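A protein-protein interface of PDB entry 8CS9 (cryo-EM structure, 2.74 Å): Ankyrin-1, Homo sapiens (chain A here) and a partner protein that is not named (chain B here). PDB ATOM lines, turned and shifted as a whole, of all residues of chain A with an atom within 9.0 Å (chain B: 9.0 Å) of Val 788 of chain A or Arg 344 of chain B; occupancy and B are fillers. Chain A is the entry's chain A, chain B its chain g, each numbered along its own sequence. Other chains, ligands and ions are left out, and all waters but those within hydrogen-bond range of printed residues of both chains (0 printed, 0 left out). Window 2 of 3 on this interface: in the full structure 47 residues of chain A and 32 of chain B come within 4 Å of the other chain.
The backbone carbonyl oxygen of Arg 346 of chain B sits at hydrogen-bond distance from the side-chain amino group of Lys 755 of chain A (2.6 Å). NZ of Lys 755 of chain A sits at hydrogen-bond distance from O of Gln 348 of chain B (2.8 Å).
The side-chain sulfur (SG) of Cys 317 of chain B sits at hydrogen-bond distance from the backbone NH (N) of Arg 346 of chain B (3.5 Å). The guanidinium group (NE) of Arg 292 of chain B is in hydrogen-bond range of the side-chain hydroxyl (OH) of Tyr 347 of chain B, 2.8 Å away. OG1 of Thr 790 of chain A is in hydrogen-bond range of O of Pro 760 of chain A (3.0 Å). The guanidinium group (NH1) of Arg 344 of chain B sits close to the side-chain amide nitrogen (NE2) of Gln 348 of chain B (3.0 Å).
Among the printed residues, merely in contact across the chains: Val 789 of chain A with Gln 348 of chain B (3.4 Å), Leu 754 of chain A with Tyr 347 of chain B (3.4 Å), Val 785 of chain A with Arg 292 of chain B (3.4 Å), Val 788 of chain A with Arg 344 of chain B (3.4 Å), Lys 755 of chain A with Tyr 347 of chain B (3.6 Å), Val 789 of chain A with Arg 344 of chain B (3.8 Å), Val 789 of chain A with Tyr 347 of chain B (3.8 Å), Val 788 of chain A with Leu 343 of chain B (3.8 Å), Val 785 of chain A with Tyr 347 of chain B (3.8 Å), Lys 755 of chain A with Ser 349 of chain B (3.9 Å), Pro 760 of chain A with Gln 348 of chain B (3.9 Å), Lys 755 of chain A with Val 293 of chain B (3.9 Å) and Leu 754 of chain A with Ser 349 of chain B (3.9 Å).
Of the printed residues of chain B, Leu 754 of chain A touches Tyr 347 (3.4 Å) and Ser 349 (3.9 Å). Of the printed residues of chain B, Val 788 of chain A touches Leu 343 (3.8 Å) and Arg 344 (3.4 Å). Val 789 of chain A touches just these residues of chain B: Arg 344 (3.8 Å), Tyr 347 (3.8 Å) and Gln 348 (3.4 Å). Of the printed residues of chain A, Leu 343 of chain B touches Val 788. Of chain A, only Val 788 and Val 789 come within 4 Å of Arg 344 of chain B. Of the printed residues of chain A, Arg 346 of chain B touches Lys 755. Of the printed residues of chain A, Ser 349 of chain B touches Leu 754 and Lys 755. The nearest printed residue of chain B that does not touch Val 788 of chain A is Tyr 347 of chain B (4.01 Å). The nearest residue of chain A that does not touch Arg 344 of chain B is Thr 790 of chain A (5.7 Å).
Of the 16 printed residues of chain B, 8 touch a printed residue of chain A. Printed residues of chain B that touch a printed residue of chain A: Arg 292, Val 293, Leu 343, Arg 344, Arg 346, Tyr 347, Gln 348 and Ser 349. Of the 19 printed residues of chain A, 6 touch a printed residue of chain B. Printed residues of chain A that touch a printed residue of chain B: Leu 754, Lys 755, Pro 760, Val 785, Val 788 and Val 789. Hydrophobic or aromatic side chains of chain A that line the printed part of chain B: Leu 754, Pro 760, Val 785, Val 788 and Val 789.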
ATOM      1  N   LEU A 754     -14.830  14.021 -15.008  1.00  0.00           N
ATOM      2  CA  LEU A 754     -13.880  13.222 -15.829  1.00  0.00           C
ATOM      3  C   LEU A 754     -13.871  13.715 -17.278  1.00  0.00           C
ATOM      4  O   LEU A 754     -12.779  13.845 -17.832  1.00  0.00           O
ATOM      5  CB  LEU A 754     -14.220  11.729 -15.767  1.00  0.00           C
ATOM      6  CG  LEU A 754     -14.004  11.043 -14.425  1.00  0.00           C
ATOM      7  CD1 LEU A 754     -14.601   9.649 -14.451  1.00  0.00           C
ATOM      8  CD2 LEU A 754     -12.526  10.981 -14.089  1.00  0.00           C
ATOM      9  N   LYS A 755     -15.027  13.974 -17.871  1.00  0.00           N
ATOM     10  CA  LYS A 755     -15.139  14.387 -19.286  1.00  0.00           C
ATOM     11  C   LYS A 755     -14.609  15.790 -19.493  1.00  0.00           C
ATOM     12  O   LYS A 755     -14.530  16.214 -20.647  1.00  0.00           O
ATOM     13  CB  LYS A 755     -16.613  14.440 -19.669  1.00  0.00           C
ATOM     14  CG  LYS A 755     -17.337  13.105 -19.700  1.00  0.00           C
ATOM     15  CD  LYS A 755     -16.763  12.171 -20.725  1.00  0.00           C
ATOM     16  CE  LYS A 755     -16.852  12.726 -22.127  1.00  0.00           C
ATOM     17  NZ  LYS A 755     -16.269  11.791 -23.114  1.00  0.00           N
ATOM     18  N   ALA A 758     -10.783  15.807 -15.449  1.00  0.00           N
ATOM     19  CA  ALA A 758     -10.427  15.497 -14.063  1.00  0.00           C
ATOM     20  C   ALA A 758      -9.509  14.295 -14.085  1.00  0.00           C
ATOM     21  O   ALA A 758      -9.654  13.467 -14.986  1.00  0.00           O
ATOM     22  CB  ALA A 758     -11.623  15.184 -13.250  1.00  0.00           C
ATOM     23  N   SER A 759      -8.596  14.227 -13.116  1.00  0.00           N
ATOM     24  CA  SER A 759      -7.619  13.133 -13.125  1.00  0.00           C
ATOM     25  C   SER A 759      -8.063  12.083 -12.130  1.00  0.00           C
ATOM     26  O   SER A 759      -8.271  12.426 -10.976  1.00  0.00           O
ATOM     27  CB  SER A 759      -6.284  13.671 -12.807  1.00  0.00           C
ATOM     28  OG  SER A 759      -6.023  14.824 -13.590  1.00  0.00           O
ATOM     29  N   PRO A 760      -8.198  10.813 -12.531  1.00  0.00           N
ATOM     30  CA  PRO A 760      -8.567   9.796 -11.591  1.00  0.00           C
ATOM     31  C   PRO A 760      -7.371   9.168 -10.872  1.00  0.00           C
ATOM     32  O   PRO A 760      -7.543   8.106 -10.317  1.00  0.00           O
ATOM     33  CB  PRO A 760      -9.209   8.780 -12.533  1.00  0.00           C
ATOM     34  CG  PRO A 760      -8.393   8.871 -13.786  1.00  0.00           C
ATOM     35  CD  PRO A 760      -8.040  10.336 -13.902  1.00  0.00           C
ATOM     36  N   ASN A 761      -6.210   9.819 -10.861  1.00  0.00           N
ATOM     37  CA  ASN A 761      -5.002   9.157 -10.298  1.00  0.00           C
ATOM     38  C   ASN A 761      -4.266  10.103  -9.370  1.00  0.00           C
ATOM     39  O   ASN A 761      -3.424   9.617  -8.619  1.00  0.00           O
ATOM     40  CB  ASN A 761      -4.087   8.652 -11.404  1.00  0.00           C
ATOM     41  CG  ASN A 761      -4.801   7.700 -12.337  1.00  0.00           C
ATOM     42  OD1 ASN A 761      -5.164   6.596 -11.942  1.00  0.00           O
ATOM     43  ND2 ASN A 761      -5.010   8.120 -13.573  1.00  0.00           N
ATOM     44  N   LEU A 771     -11.044   7.182  -6.118  1.00  0.00           N
ATOM     45  CA  LEU A 771     -11.725   5.860  -6.193  1.00  0.00           C
ATOM     46  C   LEU A 771     -11.644   5.141  -4.851  1.00  0.00           C
ATOM     47  O   LEU A 771     -12.691   4.681  -4.375  1.00  0.00           O
ATOM     48  CB  LEU A 771     -11.076   5.004  -7.278  1.00  0.00           C
ATOM     49  CG  LEU A 771     -11.553   3.559  -7.364  1.00  0.00           C
ATOM     50  CD1 LEU A 771     -13.067   3.490  -7.358  1.00  0.00           C
ATOM     51  CD2 LEU A 771     -10.995   2.890  -8.607  1.00  0.00           C
ATOM     52  N   SER A 781     -22.026   2.782  -7.785  1.00  0.00           N
ATOM     53  CA  SER A 781     -22.098   3.496  -9.056  1.00  0.00           C
ATOM     54  C   SER A 781     -20.868   4.367  -9.284  1.00  0.00           C
ATOM     55  O   SER A 781     -20.336   4.412 -10.399  1.00  0.00           O
ATOM     56  CB  SER A 781     -23.370   4.339  -9.108  1.00  0.00           C
ATOM     57  OG  SER A 781     -24.505   3.568  -8.761  1.00  0.00           O
ATOM     58  N   VAL A 782     -20.409   5.072  -8.249  1.00  0.00           N
ATOM     59  CA  VAL A 782     -19.215   5.902  -8.395  1.00  0.00           C
ATOM     60  C   VAL A 782     -17.980   5.028  -8.566  1.00  0.00           C
ATOM     61  O   VAL A 782     -17.071   5.358  -9.336  1.00  0.00           O
ATOM     62  CB  VAL A 782     -19.078   6.861  -7.199  1.00  0.00           C
ATOM     63  CG1 VAL A 782     -17.892   7.781  -7.393  1.00  0.00           C
ATOM     64  CG2 VAL A 782     -20.343   7.671  -7.030  1.00  0.00           C
ATOM     65  N   THR A 783     -17.925   3.903  -7.850  1.00  0.00           N
ATOM     66  CA  THR A 783     -16.813   2.970  -8.015  1.00  0.00           C
ATOM     67  C   THR A 783     -16.790   2.384  -9.421  1.00  0.00           C
ATOM     68  O   THR A 783     -15.720   2.239 -10.020  1.00  0.00           O
ATOM     69  CB  THR A 783     -16.904   1.851  -6.977  1.00  0.00           C
ATOM     70  OG1 THR A 783     -17.008   2.422  -5.668  1.00  0.00           O
ATOM     71  CG2 THR A 783     -15.674   0.960  -7.037  1.00  0.00           C
ATOM     72  N   ASP A 784     -17.962   2.047  -9.963  1.00  0.00           N
ATOM     73  CA  ASP A 784     -18.024   1.457 -11.298  1.00  0.00           C
ATOM     74  C   ASP A 784     -17.515   2.422 -12.362  1.00  0.00           C
ATOM     75  O   ASP A 784     -16.799   2.017 -13.284  1.00  0.00           O
ATOM     76  CB  ASP A 784     -19.454   1.025 -11.611  1.00  0.00           C
ATOM     77  CG  ASP A 784     -19.645  -0.474 -11.508  1.00  0.00           C
ATOM     78  OD1 ASP A 784     -18.646  -1.212 -11.650  1.00  0.00           O
ATOM     79  OD2 ASP A 784     -20.791  -0.915 -11.286  1.00  0.00           O
ATOM     80  N   VAL A 785     -17.836   3.705 -12.243  1.00  0.00           N
ATOM     81  CA  VAL A 785     -17.414   4.668 -13.285  1.00  0.00           C
ATOM     82  C   VAL A 785     -15.936   4.958 -13.099  1.00  0.00           C
ATOM     83  O   VAL A 785     -15.222   4.872 -14.085  1.00  0.00           O
ATOM     84  CB  VAL A 785     -18.258   5.946 -13.227  1.00  0.00           C
ATOM     85  CG1 VAL A 785     -17.653   7.073 -14.044  1.00  0.00           C
ATOM     86  CG2 VAL A 785     -19.693   5.685 -13.646  1.00  0.00           C
ATOM     87  N   LEU A 786     -15.497   5.245 -11.881  1.00  0.00           N
ATOM     88  CA  LEU A 786     -14.093   5.590 -11.556  1.00  0.00           C
ATOM     89  C   LEU A 786     -13.194   4.363 -11.673  1.00  0.00           C
ATOM     90  O   LEU A 786     -11.990   4.562 -11.793  1.00  0.00           O
ATOM     91  CB  LEU A 786     -14.081   6.167 -10.139  1.00  0.00           C
ATOM     92  CG  LEU A 786     -14.258   7.677 -10.022  1.00  0.00           C
ATOM     93  CD1 LEU A 786     -14.242   8.097  -8.566  1.00  0.00           C
ATOM     94  CD2 LEU A 786     -13.181   8.416 -10.790  1.00  0.00           C
ATOM     95  N   LYS A 787     -13.748   3.148 -11.652  1.00  0.00           N
ATOM     96  CA  LYS A 787     -12.955   1.901 -11.856  1.00  0.00           C
ATOM     97  C   LYS A 787     -12.444   1.806 -13.298  1.00  0.00           C
ATOM     98  O   LYS A 787     -11.318   1.353 -13.489  1.00  0.00           O
ATOM     99  CB  LYS A 787     -13.783   0.667 -11.520  1.00  0.00           C
ATOM    100  CG  LYS A 787     -13.004  -0.491 -10.915  1.00  0.00           C
ATOM    101  CD  LYS A 787     -13.859  -1.375 -10.035  1.00  0.00           C
ATOM    102  CE  LYS A 787     -15.134  -1.825 -10.716  1.00  0.00           C
ATOM    103  NZ  LYS A 787     -16.010  -2.584  -9.795  1.00  0.00           N
ATOM    104  N   VAL A 788     -13.250   2.200 -14.276  1.00  0.00           N
ATOM    105  CA  VAL A 788     -12.848   2.146 -15.709  1.00  0.00           C
ATOM    106  C   VAL A 788     -11.675   3.091 -15.950  1.00  0.00           C
ATOM    107  O   VAL A 788     -10.723   2.659 -16.594  1.00  0.00           O
ATOM    108  CB  VAL A 788     -14.046   2.504 -16.606  1.00  0.00           C
ATOM    109  CG1 VAL A 788     -13.661   2.694 -18.059  1.00  0.00           C
ATOM    110  CG2 VAL A 788     -15.184   1.513 -16.456  1.00  0.00           C
ATOM    111  N   VAL A 789     -11.704   4.298 -15.403  1.00  0.00           N
ATOM    112  CA  VAL A 789     -10.693   5.334 -15.748  1.00  0.00           C
ATOM    113  C   VAL A 789      -9.494   5.282 -14.803  1.00  0.00           C
ATOM    114  O   VAL A 789      -8.514   5.967 -15.094  1.00  0.00           O
ATOM    115  CB  VAL A 789     -11.362   6.722 -15.745  1.00  0.00           C
ATOM    116  CG1 VAL A 789     -12.334   6.886 -16.899  1.00  0.00           C
ATOM    117  CG2 VAL A 789     -12.056   7.004 -14.427  1.00  0.00           C
ATOM    118  N   THR A 790      -9.557   4.511 -13.725  1.00  0.00           N
ATOM    119  CA  THR A 790      -8.461   4.524 -12.720  1.00  0.00           C
ATOM    120  C   THR A 790      -7.558   3.312 -12.925  1.00  0.00           C
ATOM    121  O   THR A 790      -8.089   2.194 -12.982  1.00  0.00           O
ATOM    122  CB  THR A 790      -8.998   4.597 -11.291  1.00  0.00           C
ATOM    123  OG1 THR A 790      -9.429   5.935 -11.053  1.00  0.00           O
ATOM    124  CG2 THR A 790      -7.963   4.219 -10.257  1.00  0.00           C
ATOM    125  N   ASP A 791      -6.244   3.528 -12.992  1.00  0.00           N
ATOM    126  CA  ASP A 791      -5.285   2.431 -13.294  1.00  0.00           C
ATOM    127  C   ASP A 791      -5.011   1.556 -12.077  1.00  0.00           C
ATOM    128  O   ASP A 791      -5.492   1.878 -10.983  1.00  0.00           O
ATOM    129  CB  ASP A 791      -3.959   3.007 -13.784  1.00  0.00           C
ATOM    130  CG  ASP A 791      -3.351   4.014 -12.825  1.00  0.00           C
ATOM    131  OD1 ASP A 791      -3.658   3.936 -11.623  1.00  0.00           O
ATOM    132  OD2 ASP A 791      -2.583   4.873 -13.293  1.00  0.00           O
ATOM    133  N   GLU A 792      -4.220   0.502 -12.277  1.00  0.00           N
ATOM    134  CA  GLU A 792      -3.938  -0.369 -11.144  1.00  0.00           C
ATOM    135  C   GLU A 792      -2.895   0.262 -10.229  1.00  0.00           C
ATOM    136  O   GLU A 792      -1.992   0.974 -10.679  1.00  0.00           O
ATOM    137  CB  GLU A 792      -3.467  -1.745 -11.628  1.00  0.00           C
ATOM    138  CG  GLU A 792      -2.040  -1.806 -12.173  1.00  0.00           C
ATOM    139  CD  GLU A 792      -1.853  -1.018 -13.457  1.00  0.00           C
ATOM    140  OE1 GLU A 792      -2.764  -1.043 -14.310  1.00  0.00           O
ATOM    141  OE2 GLU A 792      -0.795  -0.371 -13.610  1.00  0.00           O
ATOM    142  N   ARG B 292     -24.751   6.676 -20.401  1.00  0.00           N
ATOM    143  CA  ARG B 292     -24.547   7.573 -19.267  1.00  0.00           C
ATOM    144  C   ARG B 292     -24.063   8.946 -19.717  1.00  0.00           C
ATOM    145  O   ARG B 292     -24.633   9.979 -19.336  1.00  0.00           O
ATOM    146  CB  ARG B 292     -23.550   6.942 -18.296  1.00  0.00           C
ATOM    147  CG  ARG B 292     -22.884   7.919 -17.351  1.00  0.00           C
ATOM    148  CD  ARG B 292     -21.746   7.254 -16.602  1.00  0.00           C
ATOM    149  NE  ARG B 292     -22.033   5.859 -16.295  1.00  0.00           N
ATOM    150  CZ  ARG B 292     -22.733   5.453 -15.245  1.00  0.00           C
ATOM    151  NH1 ARG B 292     -23.244   6.312 -14.381  1.00  0.00           N
ATOM    152  NH2 ARG B 292     -22.926   4.150 -15.060  1.00  0.00           N
ATOM    153  N   VAL B 293     -23.012   8.972 -20.540  1.00  0.00           N
ATOM    154  CA  VAL B 293     -22.426  10.236 -20.966  1.00  0.00           C
ATOM    155  C   VAL B 293     -23.416  11.040 -21.793  1.00  0.00           C
ATOM    156  O   VAL B 293     -23.557  12.252 -21.591  1.00  0.00           O
ATOM    157  CB  VAL B 293     -21.116   9.986 -21.736  1.00  0.00           C
ATOM    158  CG1 VAL B 293     -20.503  11.298 -22.181  1.00  0.00           C
ATOM    159  CG2 VAL B 293     -20.138   9.207 -20.879  1.00  0.00           C
ATOM    160  N   CYS B 317     -16.620   5.516 -29.660  1.00  0.00           N
ATOM    161  CA  CYS B 317     -16.368   4.430 -28.725  1.00  0.00           C
ATOM    162  C   CYS B 317     -17.312   3.255 -28.943  1.00  0.00           C
ATOM    163  O   CYS B 317     -17.477   2.418 -28.052  1.00  0.00           O
ATOM    164  CB  CYS B 317     -16.461   4.948 -27.292  1.00  0.00           C
ATOM    165  SG  CYS B 317     -15.437   6.405 -27.014  1.00  0.00           S
ATOM    166  N   PRO B 337     -10.217  -6.344 -24.056  1.00  0.00           N
ATOM    167  CA  PRO B 337      -9.457  -5.091 -23.905  1.00  0.00           C
ATOM    168  C   PRO B 337      -9.958  -3.972 -24.795  1.00  0.00           C
ATOM    169  O   PRO B 337      -9.897  -2.803 -24.396  1.00  0.00           O
ATOM    170  CB  PRO B 337      -8.025  -5.499 -24.275  1.00  0.00           C
ATOM    171  CG  PRO B 337      -7.974  -6.950 -24.066  1.00  0.00           C
ATOM    172  CD  PRO B 337      -9.322  -7.456 -24.434  1.00  0.00           C
ATOM    173  N   VAL B 338     -10.458  -4.299 -25.988  1.00  0.00           N
ATOM    174  CA  VAL B 338     -10.943  -3.267 -26.901  1.00  0.00           C
ATOM    175  C   VAL B 338     -12.160  -2.568 -26.314  1.00  0.00           C
ATOM    176  O   VAL B 338     -12.256  -1.336 -26.327  1.00  0.00           O
ATOM    177  CB  VAL B 338     -11.248  -3.874 -28.281  1.00  0.00           C
ATOM    178  CG1 VAL B 338     -11.691  -2.793 -29.242  1.00  0.00           C
ATOM    179  CG2 VAL B 338     -10.028  -4.598 -28.817  1.00  0.00           C
ATOM    180  N   GLN B 339     -13.102  -3.346 -25.779  1.00  0.00           N
ATOM    181  CA  GLN B 339     -14.288  -2.756 -25.169  1.00  0.00           C
ATOM    182  C   GLN B 339     -13.930  -1.975 -23.911  1.00  0.00           C
ATOM    183  O   GLN B 339     -14.488  -0.897 -23.662  1.00  0.00           O
ATOM    184  CB  GLN B 339     -15.313  -3.842 -24.857  1.00  0.00           C
ATOM    185  CG  GLN B 339     -16.587  -3.308 -24.239  1.00  0.00           C
ATOM    186  CD  GLN B 339     -17.318  -4.349 -23.432  1.00  0.00           C
ATOM    187  OE1 GLN B 339     -17.152  -5.548 -23.651  1.00  0.00           O
ATOM    188  NE2 GLN B 339     -18.130  -3.900 -22.485  1.00  0.00           N
ATOM    189  N   ARG B 340     -12.996  -2.497 -23.108  1.00  0.00           N
ATOM    190  CA  ARG B 340     -12.561  -1.762 -21.923  1.00  0.00           C
ATOM    191  C   ARG B 340     -11.941  -0.418 -22.285  1.00  0.00           C
ATOM    192  O   ARG B 340     -12.261   0.603 -21.665  1.00  0.00           O
ATOM    193  CB  ARG B 340     -11.567  -2.595 -21.120  1.00  0.00           C
ATOM    194  CG  ARG B 340     -12.165  -3.808 -20.448  1.00  0.00           C
ATOM    195  CD  ARG B 340     -11.773  -3.865 -18.983  1.00  0.00           C
ATOM    196  NE  ARG B 340     -12.432  -4.967 -18.294  1.00  0.00           N
ATOM    197  CZ  ARG B 340     -12.073  -6.238 -18.404  1.00  0.00           C
ATOM    198  NH1 ARG B 340     -11.031  -6.601 -19.133  1.00  0.00           N
ATOM    199  NH2 ARG B 340     -12.774  -7.167 -17.761  1.00  0.00           N
ATOM    200  N   GLU B 341     -11.067  -0.392 -23.290  1.00  0.00           N
ATOM    201  CA  GLU B 341     -10.438   0.853 -23.703  1.00  0.00           C
ATOM    202  C   GLU B 341     -11.415   1.811 -24.368  1.00  0.00           C
ATOM    203  O   GLU B 341     -11.294   3.025 -24.175  1.00  0.00           O
ATOM    204  CB  GLU B 341      -9.261   0.568 -24.642  1.00  0.00           C
ATOM    205  CG  GLU B 341      -8.615   1.811 -25.233  1.00  0.00           C
ATOM    206  CD  GLU B 341      -7.821   2.604 -24.214  1.00  0.00           C
ATOM    207  OE1 GLU B 341      -7.444   2.030 -23.171  1.00  0.00           O
ATOM    208  OE2 GLU B 341      -7.574   3.805 -24.454  1.00  0.00           O
ATOM    209  N   LEU B 342     -12.388   1.307 -25.125  1.00  0.00           N
ATOM    210  CA  LEU B 342     -13.422   2.177 -25.671  1.00  0.00           C
ATOM    211  C   LEU B 342     -14.300   2.791 -24.585  1.00  0.00           C
ATOM    212  O   LEU B 342     -14.657   3.968 -24.691  1.00  0.00           O
ATOM    213  CB  LEU B 342     -14.273   1.405 -26.681  1.00  0.00           C
ATOM    214  CG  LEU B 342     -13.587   1.116 -28.020  1.00  0.00           C
ATOM    215  CD1 LEU B 342     -14.446   0.229 -28.897  1.00  0.00           C
ATOM    216  CD2 LEU B 342     -13.236   2.400 -28.740  1.00  0.00           C
ATOM    217  N   LEU B 343     -14.540   2.093 -23.484  1.00  0.00           N
ATOM    218  CA  LEU B 343     -15.297   2.692 -22.362  1.00  0.00           C
ATOM    219  C   LEU B 343     -14.454   3.749 -21.668  1.00  0.00           C
ATOM    220  O   LEU B 343     -15.002   4.814 -21.398  1.00  0.00           O
ATOM    221  CB  LEU B 343     -15.754   1.631 -21.366  1.00  0.00           C
ATOM    222  CG  LEU B 343     -16.816   2.075 -20.367  1.00  0.00           C
ATOM    223  CD1 LEU B 343     -17.956   2.803 -21.060  1.00  0.00           C
ATOM    224  CD2 LEU B 343     -17.340   0.885 -19.586  1.00  0.00           C
ATOM    225  N   ARG B 344     -13.178   3.493 -21.414  1.00  0.00           N
ATOM    226  CA  ARG B 344     -12.283   4.513 -20.813  1.00  0.00           C
ATOM    227  C   ARG B 344     -12.248   5.739 -21.711  1.00  0.00           C
ATOM    228  O   ARG B 344     -12.087   6.842 -21.204  1.00  0.00           O
ATOM    229  CB  ARG B 344     -10.883   3.941 -20.601  1.00  0.00           C
ATOM    230  CG  ARG B 344     -10.128   4.534 -19.422  1.00  0.00           C
ATOM    231  CD  ARG B 344      -8.777   5.070 -19.848  1.00  0.00           C
ATOM    232  NE  ARG B 344      -8.937   6.157 -20.798  1.00  0.00           N
ATOM    233  CZ  ARG B 344      -8.361   7.346 -20.688  1.00  0.00           C
ATOM    234  NH1 ARG B 344      -7.567   7.606 -19.664  1.00  0.00           N
ATOM    235  NH2 ARG B 344      -8.580   8.274 -21.602  1.00  0.00           N
ATOM    236  N   ARG B 345     -12.412   5.546 -23.002  1.00  0.00           N
ATOM    237  CA  ARG B 345     -12.326   6.669 -23.954  1.00  0.00           C
ATOM    238  C   ARG B 345     -13.642   7.465 -23.959  1.00  0.00           C
ATOM    239  O   ARG B 345     -13.582   8.645 -24.316  1.00  0.00           O
ATOM    240  CB  ARG B 345     -11.897   6.094 -25.306  1.00  0.00           C
ATOM    241  CG  ARG B 345     -10.393   5.968 -25.487  1.00  0.00           C
ATOM    242  CD  ARG B 345     -10.052   6.031 -26.960  1.00  0.00           C
ATOM    243  NE  ARG B 345     -11.277   6.067 -27.739  1.00  0.00           N
ATOM    244  CZ  ARG B 345     -11.452   5.442 -28.893  1.00  0.00           C
ATOM    245  NH1 ARG B 345     -10.470   4.727 -29.415  1.00  0.00           N
ATOM    246  NH2 ARG B 345     -12.606   5.533 -29.524  1.00  0.00           N
ATOM    247  N   ARG B 346     -14.780   6.852 -23.600  1.00  0.00           N
ATOM    248  CA  ARG B 346     -16.074   7.576 -23.489  1.00  0.00           C
ATOM    249  C   ARG B 346     -16.146   8.231 -22.116  1.00  0.00           C
ATOM    250  O   ARG B 346     -16.515   9.391 -22.069  1.00  0.00           O
ATOM    251  CB  ARG B 346     -17.274   6.669 -23.746  1.00  0.00           C
ATOM    252  CG  ARG B 346     -18.620   7.364 -23.688  1.00  0.00           C
ATOM    253  CD  ARG B 346     -19.188   7.498 -25.076  1.00  0.00           C
ATOM    254  NE  ARG B 346     -20.454   8.202 -25.085  1.00  0.00           N
ATOM    255  CZ  ARG B 346     -20.570   9.512 -25.184  1.00  0.00           C
ATOM    256  NH1 ARG B 346     -19.488  10.263 -25.266  1.00  0.00           N
ATOM    257  NH2 ARG B 346     -21.763  10.070 -25.194  1.00  0.00           N
ATOM    258  N   TYR B 347     -15.724   7.537 -21.062  1.00  0.00           N
ATOM    259  CA  TYR B 347     -15.813   8.061 -19.682  1.00  0.00           C
ATOM    260  C   TYR B 347     -14.766   9.164 -19.509  1.00  0.00           C
ATOM    261  O   TYR B 347     -14.923   9.963 -18.592  1.00  0.00           O
ATOM    262  CB  TYR B 347     -15.694   6.899 -18.696  1.00  0.00           C
ATOM    263  CG  TYR B 347     -16.953   6.129 -18.426  1.00  0.00           C
ATOM    264  CD1 TYR B 347     -16.961   5.099 -17.506  1.00  0.00           C
ATOM    265  CD2 TYR B 347     -18.127   6.430 -19.085  1.00  0.00           C
ATOM    266  CE1 TYR B 347     -18.110   4.377 -17.245  1.00  0.00           C
ATOM    267  CE2 TYR B 347     -19.286   5.721 -18.838  1.00  0.00           C
ATOM    268  CZ  TYR B 347     -19.275   4.692 -17.917  1.00  0.00           C
ATOM    269  OH  TYR B 347     -20.414   3.993 -17.660  1.00  0.00           O
ATOM    270  N   GLN B 348     -13.751   9.211 -20.371  1.00  0.00           N
ATOM    271  CA  GLN B 348     -12.656  10.212 -20.294  1.00  0.00           C
ATOM    272  C   GLN B 348     -12.869  11.249 -21.383  1.00  0.00           C
ATOM    273  O   GLN B 348     -13.761  11.037 -22.215  1.00  0.00           O
ATOM    274  CB  GLN B 348     -11.297   9.575 -20.516  1.00  0.00           C
ATOM    275  CG  GLN B 348     -10.833   8.693 -19.366  1.00  0.00           C
ATOM    276  CD  GLN B 348     -10.101   9.437 -18.275  1.00  0.00           C
ATOM    277  OE1 GLN B 348     -10.271  10.639 -18.088  1.00  0.00           O
ATOM    278  NE2 GLN B 348      -9.281   8.712 -17.532  1.00  0.00           N
ATOM    279  N   SER B 349     -12.093  12.319 -21.394  1.00  0.00           N
ATOM    280  CA  SER B 349     -12.396  13.417 -22.350  1.00  0.00           C
ATOM    281  C   SER B 349     -12.452  12.880 -23.785  1.00  0.00           C
ATOM    282  O   SER B 349     -12.839  13.662 -24.681  1.00  0.00           O
ATOM    283  CB  SER B 349     -11.421  14.552 -22.201  1.00  0.00           C
